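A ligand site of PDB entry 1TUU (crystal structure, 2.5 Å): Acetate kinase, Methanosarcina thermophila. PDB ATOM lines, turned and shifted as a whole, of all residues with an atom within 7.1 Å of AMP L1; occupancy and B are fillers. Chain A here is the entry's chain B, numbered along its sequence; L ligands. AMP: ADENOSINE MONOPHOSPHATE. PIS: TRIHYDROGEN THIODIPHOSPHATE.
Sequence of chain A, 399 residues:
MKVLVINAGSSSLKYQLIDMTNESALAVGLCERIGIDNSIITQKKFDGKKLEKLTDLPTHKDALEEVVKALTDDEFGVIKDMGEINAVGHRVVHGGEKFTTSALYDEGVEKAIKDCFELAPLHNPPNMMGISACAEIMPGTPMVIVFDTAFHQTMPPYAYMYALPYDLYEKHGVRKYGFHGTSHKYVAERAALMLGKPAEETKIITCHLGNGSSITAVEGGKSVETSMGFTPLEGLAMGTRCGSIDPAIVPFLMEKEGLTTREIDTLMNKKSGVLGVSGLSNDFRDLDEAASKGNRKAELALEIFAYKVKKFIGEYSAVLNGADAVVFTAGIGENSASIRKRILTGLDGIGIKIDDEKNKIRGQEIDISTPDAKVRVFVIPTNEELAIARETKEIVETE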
ATOM      1  N   HIS A 208     -22.776  18.386 -33.382  1.00  0.00           N
ATOM      2  CA  HIS A 208     -22.192  18.601 -32.058  1.00  0.00           C
ATOM      3  C   HIS A 208     -23.244  19.348 -31.234  1.00  0.00           C
ATOM      4  O   HIS A 208     -23.423  20.553 -31.376  1.00  0.00           O
ATOM      5  CB  HIS A 208     -20.923  19.448 -32.183  1.00  0.00           C
ATOM      6  CG  HIS A 208     -20.251  19.724 -30.875  1.00  0.00           C
ATOM      7  ND1 HIS A 208     -19.222  18.949 -30.377  1.00  0.00           N
ATOM      8  CD2 HIS A 208     -20.485  20.679 -29.941  1.00  0.00           C
ATOM      9  CE1 HIS A 208     -18.855  19.415 -29.201  1.00  0.00           C
ATOM     10  NE2 HIS A 208     -19.606  20.459 -28.913  1.00  0.00           N
ATOM     11  N   LEU A 209     -23.924  18.603 -30.367  1.00  0.00           N
ATOM     12  CA  LEU A 209     -24.969  19.175 -29.532  1.00  0.00           C
ATOM     13  C   LEU A 209     -24.604  19.239 -28.050  1.00  0.00           C
ATOM     14  O   LEU A 209     -24.629  18.223 -27.347  1.00  0.00           O
ATOM     15  CB  LEU A 209     -26.256  18.365 -29.702  1.00  0.00           C
ATOM     16  CG  LEU A 209     -26.650  18.067 -31.153  1.00  0.00           C
ATOM     17  CD1 LEU A 209     -28.042  17.474 -31.189  1.00  0.00           C
ATOM     18  CD2 LEU A 209     -26.593  19.333 -31.981  1.00  0.00           C
ATOM     19  N   GLY A 210     -24.279  20.451 -27.596  1.00  0.00           N
ATOM     20  CA  GLY A 210     -23.902  20.680 -26.214  1.00  0.00           C
ATOM     21  C   GLY A 210     -24.414  22.042 -25.749  1.00  0.00           C
ATOM     22  O   GLY A 210     -25.390  22.546 -26.313  1.00  0.00           O
ATOM     23  N   ASN A 211     -23.791  22.641 -24.728  1.00  0.00           N
ATOM     24  CA  ASN A 211     -24.267  23.952 -24.271  1.00  0.00           C
ATOM     25  C   ASN A 211     -24.275  24.859 -25.469  1.00  0.00           C
ATOM     26  O   ASN A 211     -25.134  25.742 -25.601  1.00  0.00           O
ATOM     27  CB  ASN A 211     -23.369  24.560 -23.195  1.00  0.00           C
ATOM     28  CG  ASN A 211     -23.934  25.869 -22.647  1.00  0.00           C
ATOM     29  OD1 ASN A 211     -25.053  25.878 -22.129  1.00  0.00           O
ATOM     30  ND2 ASN A 211     -23.195  26.964 -22.781  1.00  0.00           N
ATOM     31  N   GLY A 212     -23.285  24.630 -26.335  1.00  0.00           N
ATOM     32  CA  GLY A 212     -23.142  25.385 -27.567  1.00  0.00           C
ATOM     33  C   GLY A 212     -23.280  24.355 -28.674  1.00  0.00           C
ATOM     34  O   GLY A 212     -22.754  23.253 -28.554  1.00  0.00           O
ATOM     35  N   GLY A 239     -27.766  26.497 -25.541  1.00  0.00           N
ATOM     36  CA  GLY A 239     -28.139  26.642 -24.133  1.00  0.00           C
ATOM     37  C   GLY A 239     -28.557  28.072 -23.785  1.00  0.00           C
ATOM     38  O   GLY A 239     -29.610  28.310 -23.216  1.00  0.00           O
ATOM     39  N   SER A 281     -34.026  26.985 -17.361  1.00  0.00           N
ATOM     40  CA  SER A 281     -32.618  26.611 -17.311  1.00  0.00           C
ATOM     41  C   SER A 281     -31.968  26.509 -18.688  1.00  0.00           C
ATOM     42  O   SER A 281     -32.647  26.358 -19.705  1.00  0.00           O
ATOM     43  CB  SER A 281     -32.482  25.280 -16.583  1.00  0.00           C
ATOM     44  OG  SER A 281     -31.244  24.646 -16.869  1.00  0.00           O
ATOM     45  N   ASN A 282     -30.642  26.590 -18.729  1.00  0.00           N
ATOM     46  CA  ASN A 282     -29.920  26.460 -19.982  1.00  0.00           C
ATOM     47  C   ASN A 282     -29.521  24.993 -20.096  1.00  0.00           C
ATOM     48  O   ASN A 282     -28.915  24.573 -21.074  1.00  0.00           O
ATOM     49  CB  ASN A 282     -28.641  27.306 -19.964  1.00  0.00           C
ATOM     50  CG  ASN A 282     -27.555  26.671 -19.134  1.00  0.00           C
ATOM     51  OD1 ASN A 282     -27.728  26.435 -17.935  1.00  0.00           O
ATOM     52  ND2 ASN A 282     -26.421  26.385 -19.756  1.00  0.00           N
ATOM     53  N   ASP A 283     -29.851  24.220 -19.059  1.00  0.00           N
ATOM     54  CA  ASP A 283     -29.529  22.802 -19.040  1.00  0.00           C
ATOM     55  C   ASP A 283     -30.640  21.980 -19.684  1.00  0.00           C
ATOM     56  O   ASP A 283     -31.773  21.981 -19.209  1.00  0.00           O
ATOM     57  CB  ASP A 283     -29.300  22.337 -17.612  1.00  0.00           C
ATOM     58  CG  ASP A 283     -28.864  20.874 -17.544  1.00  0.00           C
ATOM     59  OD1 ASP A 283     -29.711  19.987 -17.732  1.00  0.00           O
ATOM     60  OD2 ASP A 283     -27.655  20.629 -17.301  1.00  0.00           O
ATOM     61  N   PHE A 284     -30.320  21.279 -20.773  1.00  0.00           N
ATOM     62  CA  PHE A 284     -31.317  20.476 -21.471  1.00  0.00           C
ATOM     63  C   PHE A 284     -31.853  19.318 -20.660  1.00  0.00           C
ATOM     64  O   PHE A 284     -33.057  19.051 -20.689  1.00  0.00           O
ATOM     65  CB  PHE A 284     -30.749  19.957 -22.803  1.00  0.00           C
ATOM     66  CG  PHE A 284     -30.549  21.033 -23.827  1.00  0.00           C
ATOM     67  CD1 PHE A 284     -29.559  22.004 -23.644  1.00  0.00           C
ATOM     68  CD2 PHE A 284     -31.355  21.103 -24.954  1.00  0.00           C
ATOM     69  CE1 PHE A 284     -29.381  23.023 -24.567  1.00  0.00           C
ATOM     70  CE2 PHE A 284     -31.186  22.118 -25.891  1.00  0.00           C
ATOM     71  CZ  PHE A 284     -30.184  23.079 -25.693  1.00  0.00           C
ATOM     72  N   ARG A 285     -30.983  18.635 -19.940  1.00  0.00           N
ATOM     73  CA  ARG A 285     -31.446  17.512 -19.124  1.00  0.00           C
ATOM     74  C   ARG A 285     -32.550  17.967 -18.167  1.00  0.00           C
ATOM     75  O   ARG A 285     -33.551  17.271 -18.025  1.00  0.00           O
ATOM     76  CB  ARG A 285     -30.276  16.895 -18.358  1.00  0.00           C
ATOM     77  CG  ARG A 285     -30.651  15.630 -17.597  1.00  0.00           C
ATOM     78  CD  ARG A 285     -29.462  15.056 -16.824  1.00  0.00           C
ATOM     79  NE  ARG A 285     -28.976  15.985 -15.805  1.00  0.00           N
ATOM     80  CZ  ARG A 285     -29.710  16.445 -14.799  1.00  0.00           C
ATOM     81  NH1 ARG A 285     -30.974  16.050 -14.663  1.00  0.00           N
ATOM     82  NH2 ARG A 285     -29.169  17.296 -13.920  1.00  0.00           N
ATOM     83  N   ASP A 286     -32.392  19.132 -17.542  1.00  0.00           N
ATOM     84  CA  ASP A 286     -33.423  19.634 -16.624  1.00  0.00           C
ATOM     85  C   ASP A 286     -34.675  20.065 -17.402  1.00  0.00           C
ATOM     86  O   ASP A 286     -35.793  19.933 -16.911  1.00  0.00           O
ATOM     87  CB  ASP A 286     -32.928  20.844 -15.805  1.00  0.00           C
ATOM     88  CG  ASP A 286     -31.805  20.480 -14.844  1.00  0.00           C
ATOM     89  OD1 ASP A 286     -31.858  19.399 -14.205  1.00  0.00           O
ATOM     90  OD2 ASP A 286     -30.874  21.305 -14.709  1.00  0.00           O
ATOM     91  N   ASP A 288     -35.636  18.743 -20.215  1.00  0.00           N
ATOM     92  CA  ASP A 288     -36.284  17.539 -20.714  1.00  0.00           C
ATOM     93  C   ASP A 288     -37.279  17.076 -19.652  1.00  0.00           C
ATOM     94  O   ASP A 288     -38.409  16.703 -19.967  1.00  0.00           O
ATOM     95  CB  ASP A 288     -35.248  16.450 -21.008  1.00  0.00           C
ATOM     96  CG  ASP A 288     -35.857  15.246 -21.725  1.00  0.00           C
ATOM     97  OD1 ASP A 288     -36.972  15.395 -22.288  1.00  0.00           O
ATOM     98  OD2 ASP A 288     -35.231  14.161 -21.738  1.00  0.00           O
ATOM     99  N   THR A 329     -23.012  13.919 -31.729  1.00  0.00           N
ATOM    100  CA  THR A 329     -21.988  13.849 -30.716  1.00  0.00           C
ATOM    101  C   THR A 329     -22.209  14.949 -29.676  1.00  0.00           C
ATOM    102  O   THR A 329     -23.213  15.664 -29.741  1.00  0.00           O
ATOM    103  CB  THR A 329     -20.578  14.017 -31.331  1.00  0.00           C
ATOM    104  OG1 THR A 329     -19.585  13.841 -30.322  1.00  0.00           O
ATOM    105  CG2 THR A 329     -20.437  15.404 -31.950  1.00  0.00           C
ATOM    106  N   ALA A 330     -21.283  15.060 -28.732  1.00  0.00           N
ATOM    107  CA  ALA A 330     -21.346  16.026 -27.633  1.00  0.00           C
ATOM    108  C   ALA A 330     -22.423  15.609 -26.624  1.00  0.00           C
ATOM    109  O   ALA A 330     -23.224  14.692 -26.884  1.00  0.00           O
ATOM    110  CB  ALA A 330     -21.604  17.440 -28.179  1.00  0.00           C
ATOM    111  N   GLY A 331     -22.449  16.293 -25.492  1.00  0.00           N
ATOM    112  CA  GLY A 331     -23.380  15.967 -24.417  1.00  0.00           C
ATOM    113  C   GLY A 331     -24.820  15.623 -24.749  1.00  0.00           C
ATOM    114  O   GLY A 331     -25.322  14.572 -24.354  1.00  0.00           O
ATOM    115  N   ILE A 332     -25.509  16.512 -25.456  1.00  0.00           N
ATOM    116  CA  ILE A 332     -26.888  16.251 -25.809  1.00  0.00           C
ATOM    117  C   ILE A 332     -26.937  15.148 -26.847  1.00  0.00           C
ATOM    118  O   ILE A 332     -27.756  14.239 -26.781  1.00  0.00           O
ATOM    119  CB  ILE A 332     -27.548  17.513 -26.392  1.00  0.00           C
ATOM    120  CG1 ILE A 332     -27.396  18.669 -25.404  1.00  0.00           C
ATOM    121  CG2 ILE A 332     -29.006  17.225 -26.700  1.00  0.00           C
ATOM    122  CD1 ILE A 332     -27.700  20.038 -25.994  1.00  0.00           C
ATOM    123  N   GLY A 333     -26.002  15.207 -27.792  1.00  0.00           N
ATOM    124  CA  GLY A 333     -25.958  14.223 -28.863  1.00  0.00           C
ATOM    125  C   GLY A 333     -25.583  12.813 -28.477  1.00  0.00           C
ATOM    126  O   GLY A 333     -25.986  11.857 -29.137  1.00  0.00           O
ATOM    127  N   GLU A 334     -24.846  12.669 -27.388  1.00  0.00           N
ATOM    128  CA  GLU A 334     -24.423  11.360 -26.925  1.00  0.00           C
ATOM    129  C   GLU A 334     -25.360  10.709 -25.925  1.00  0.00           C
ATOM    130  O   GLU A 334     -25.549   9.489 -25.959  1.00  0.00           O
ATOM    131  CB  GLU A 334     -23.044  11.469 -26.293  1.00  0.00           C
ATOM    132  CG  GLU A 334     -21.950  11.844 -27.234  1.00  0.00           C
ATOM    133  CD  GLU A 334     -20.645  12.116 -26.519  1.00  0.00           C
ATOM    134  OE1 GLU A 334     -20.342  11.375 -25.559  1.00  0.00           O
ATOM    135  OE2 GLU A 334     -19.939  13.076 -26.919  1.00  0.00           O
ATOM    136  N   ASN A 335     -25.955  11.522 -25.053  1.00  0.00           N
ATOM    137  CA  ASN A 335     -26.819  10.975 -24.016  1.00  0.00           C
ATOM    138  C   ASN A 335     -28.310  11.280 -24.084  1.00  0.00           C
ATOM    139  O   ASN A 335     -29.055  10.871 -23.215  1.00  0.00           O
ATOM    140  CB  ASN A 335     -26.313  11.446 -22.636  1.00  0.00           C
ATOM    141  CG  ASN A 335     -24.793  11.505 -22.543  1.00  0.00           C
ATOM    142  OD1 ASN A 335     -24.107  10.488 -22.640  1.00  0.00           O
ATOM    143  ND2 ASN A 335     -24.278  12.705 -22.341  1.00  0.00           N
ATOM    144  N   SER A 336     -28.783  11.976 -25.108  1.00  0.00           N
ATOM    145  CA  SER A 336     -30.211  12.265 -25.133  1.00  0.00           C
ATOM    146  C   SER A 336     -31.014  11.587 -26.232  1.00  0.00           C
ATOM    147  O   SER A 336     -31.163  12.124 -27.337  1.00  0.00           O
ATOM    148  CB  SER A 336     -30.454  13.778 -25.178  1.00  0.00           C
ATOM    149  OG  SER A 336     -31.846  14.044 -25.163  1.00  0.00           O
ATOM    150  N   ALA A 337     -31.525  10.409 -25.916  1.00  0.00           N
ATOM    151  CA  ALA A 337     -32.317   9.651 -26.860  1.00  0.00           C
ATOM    152  C   ALA A 337     -33.674  10.337 -26.972  1.00  0.00           C
ATOM    153  O   ALA A 337     -34.491   9.964 -27.812  1.00  0.00           O
ATOM    154  CB  ALA A 337     -32.491   8.230 -26.355  1.00  0.00           C
ATOM    155  N   SER A 338     -33.892  11.339 -26.146  1.00  0.00           N
ATOM    156  CA  SER A 338     -35.133  12.097 -26.137  1.00  0.00           C
ATOM    157  C   SER A 338     -35.090  13.129 -27.251  1.00  0.00           C
ATOM    158  O   SER A 338     -35.923  13.121 -28.163  1.00  0.00           O
ATOM    159  CB  SER A 338     -35.301  12.775 -24.776  1.00  0.00           C
ATOM    160  OG  SER A 338     -36.379  13.690 -24.753  1.00  0.00           O
ATOM    161  N   ILE A 339     -34.090  13.989 -27.190  1.00  0.00           N
ATOM    162  CA  ILE A 339     -33.923  15.028 -28.186  1.00  0.00           C
ATOM    163  C   ILE A 339     -33.586  14.455 -29.566  1.00  0.00           C
ATOM    164  O   ILE A 339     -34.116  14.945 -30.569  1.00  0.00           O
ATOM    165  CB  ILE A 339     -32.835  16.020 -27.739  1.00  0.00           C
ATOM    166  CG1 ILE A 339     -33.303  16.710 -26.450  1.00  0.00           C
ATOM    167  CG2 ILE A 339     -32.565  17.051 -28.825  1.00  0.00           C
ATOM    168  CD1 ILE A 339     -32.361  17.749 -25.913  1.00  0.00           C
ATOM    169  N   ARG A 362     -26.830   4.771 -24.428  1.00  0.00           N
ATOM    170  CA  ARG A 362     -26.089   6.009 -24.178  1.00  0.00           C
ATOM    171  C   ARG A 362     -24.585   5.834 -24.358  1.00  0.00           C
ATOM    172  O   ARG A 362     -24.036   4.744 -24.165  1.00  0.00           O
ATOM    173  CB  ARG A 362     -26.346   6.548 -22.774  1.00  0.00           C
ATOM    174  CG  ARG A 362     -27.742   7.090 -22.526  1.00  0.00           C
ATOM    175  CD  ARG A 362     -27.793   7.842 -21.200  1.00  0.00           C
ATOM    176  NE  ARG A 362     -29.149   8.293 -20.865  1.00  0.00           N
ATOM    177  CZ  ARG A 362     -29.449   9.000 -19.774  1.00  0.00           C
ATOM    178  NH1 ARG A 362     -28.481   9.314 -18.916  1.00  0.00           N
ATOM    179  NH2 ARG A 362     -30.708   9.358 -19.545  1.00  0.00           N
HETATM  180  P   AMP L   1     -21.067  19.760 -23.115  1.00  0.00           P
HETATM  181  O1P AMP L   1     -20.413  21.019 -22.768  1.00  0.00           O
HETATM  182  O2P AMP L   1     -20.449  18.557 -22.475  1.00  0.00           O
HETATM  183  O3P AMP L   1     -21.230  19.581 -24.622  1.00  0.00           O
HETATM  184  O5' AMP L   1     -22.549  19.907 -22.462  1.00  0.00           O
HETATM  185  C5' AMP L   1     -23.452  18.813 -22.643  1.00  0.00           C
HETATM  186  C4' AMP L   1     -24.838  19.457 -22.627  1.00  0.00           C
HETATM  187  O4' AMP L   1     -25.817  18.383 -22.845  1.00  0.00           O
HETATM  188  C3' AMP L   1     -25.186  20.189 -21.165  1.00  0.00           C
HETATM  189  O3' AMP L   1     -25.717  21.545 -21.492  1.00  0.00           O
HETATM  190  C2' AMP L   1     -26.268  19.176 -20.564  1.00  0.00           C
HETATM  191  O2' AMP L   1     -27.389  19.836 -20.012  1.00  0.00           O
HETATM  192  C1' AMP L   1     -26.780  18.288 -21.808  1.00  0.00           C
HETATM  193  N9  AMP L   1     -26.928  16.879 -21.415  1.00  0.00           N
HETATM  194  C8  AMP L   1     -25.965  15.993 -20.882  1.00  0.00           C
HETATM  195  N7  AMP L   1     -26.365  14.732 -20.614  1.00  0.00           N
HETATM  196  C5  AMP L   1     -27.709  14.837 -21.019  1.00  0.00           C
HETATM  197  C6  AMP L   1     -28.764  13.873 -21.066  1.00  0.00           C
HETATM  198  N6  AMP L   1     -28.519  12.597 -20.586  1.00  0.00           N
HETATM  199  N1  AMP L   1     -30.003  14.325 -21.552  1.00  0.00           N
HETATM  200  C2  AMP L   1     -30.194  15.589 -22.012  1.00  0.00           C
HETATM  201  N3  AMP L   1     -29.250  16.554 -22.011  1.00  0.00           N
HETATM  202  C4  AMP L   1     -28.047  16.126 -21.551  1.00  0.00           C
HETATM  203  P1  PIS L   2     -19.090  24.078 -25.781  1.00  0.00           P
HETATM  204  O1  PIS L   2     -19.767  25.217 -26.636  1.00  0.00           O
HETATM  205  P2  PIS L   2     -19.236  26.683 -27.187  1.00  0.00           P
HETATM  206  S1  PIS L   2     -20.402  27.286 -27.952  1.00  0.00           S
HETATM  207  O2  PIS L   2     -18.333  24.377 -24.572  1.00  0.00           O
HETATM  208  O3  PIS L   2     -19.673  22.706 -25.958  1.00  0.00           O
HETATM  209  O4  PIS L   2     -18.837  27.512 -26.015  1.00  0.00           O
HETATM  210  O5  PIS L   2     -20.315  24.408 -24.949  1.00  0.00           O
HETATM  211  O6  PIS L   2     -18.076  26.483 -28.189  1.00  0.00           O
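Gly 210 touches AMP L1.
Asn 211 touches AMP L1.
Gly 331 touches AMP L1.
Ser 336 touches AMP L1 (CB to C2, 3.7 Å).
NH1 of Arg 362 touches N6 of AMP L1, 3.7 Å away.
Hydrophobic or aromatic side chains within 4 Å of AMP L1: Phe 284 and Ile 332.
Along chain A the residues within 4 Å of AMP L1 span positions 210 to 362.
The nearest printed residue that does not touch AMP L1 is Ala 330 (4.2 Å).
The side-chain carboxylate (OD2) of Asp 283 is in hydrogen-bond range of an oxygen (O2') of AMP L1 (2.8 Å).
An oxygen (O4') of AMP L1 sits close to the backbone NH (N) of Ile 332 (3.2 Å).
A nitrogen (N7) of AMP L1 lies within hydrogen-bond range of the side-chain amide nitrogen (ND2) of Asn 335 (3.4 Å).
The backbone NH (N) of Phe 284 is in hydrogen-bond range of an oxygen (O2') of AMP L1 (3.4 Å).
N of Gly 212 is in hydrogen-bond range of O5 of PIS L2 (3.3 Å).
A nitrogen (N3) of AMP L1 lies within hydrogen-bond range of the backbone NH (N) of Arg 285 (3.4 Å).
The backbone carbonyl oxygen (O) of Asn 335 is in hydrogen-bond range of a nitrogen (N6) of AMP L1 (3.2 Å).
OD1 of Asp 286 is in salt-bridge range of NH2 of Arg 285, 3.4 Å away.
N of Ile 332 sits at hydrogen-bond distance from O of Leu 209 (2.7 Å).
OD1 of Asp 283 is in hydrogen-bond range of N of Asp 286.
N of Gly 331 is in hydrogen-bond range of O of Leu 209 (3.5 Å).
The side-chain carboxylate (OD1) of Asp 283 is in hydrogen-bond range of the backbone NH (N) of Arg 285.
OG of Ser 336 is in hydrogen-bond range of N of Ile 339.
O of Asn 335 lies within hydrogen-bond range of NE of Arg 362, at 3.5 Å.
The side-chain amide oxygen (OD1) of Asn 211 lies within hydrogen-bond range of the side-chain amide nitrogen (ND2) of Asn 282, 2.8 Å away.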
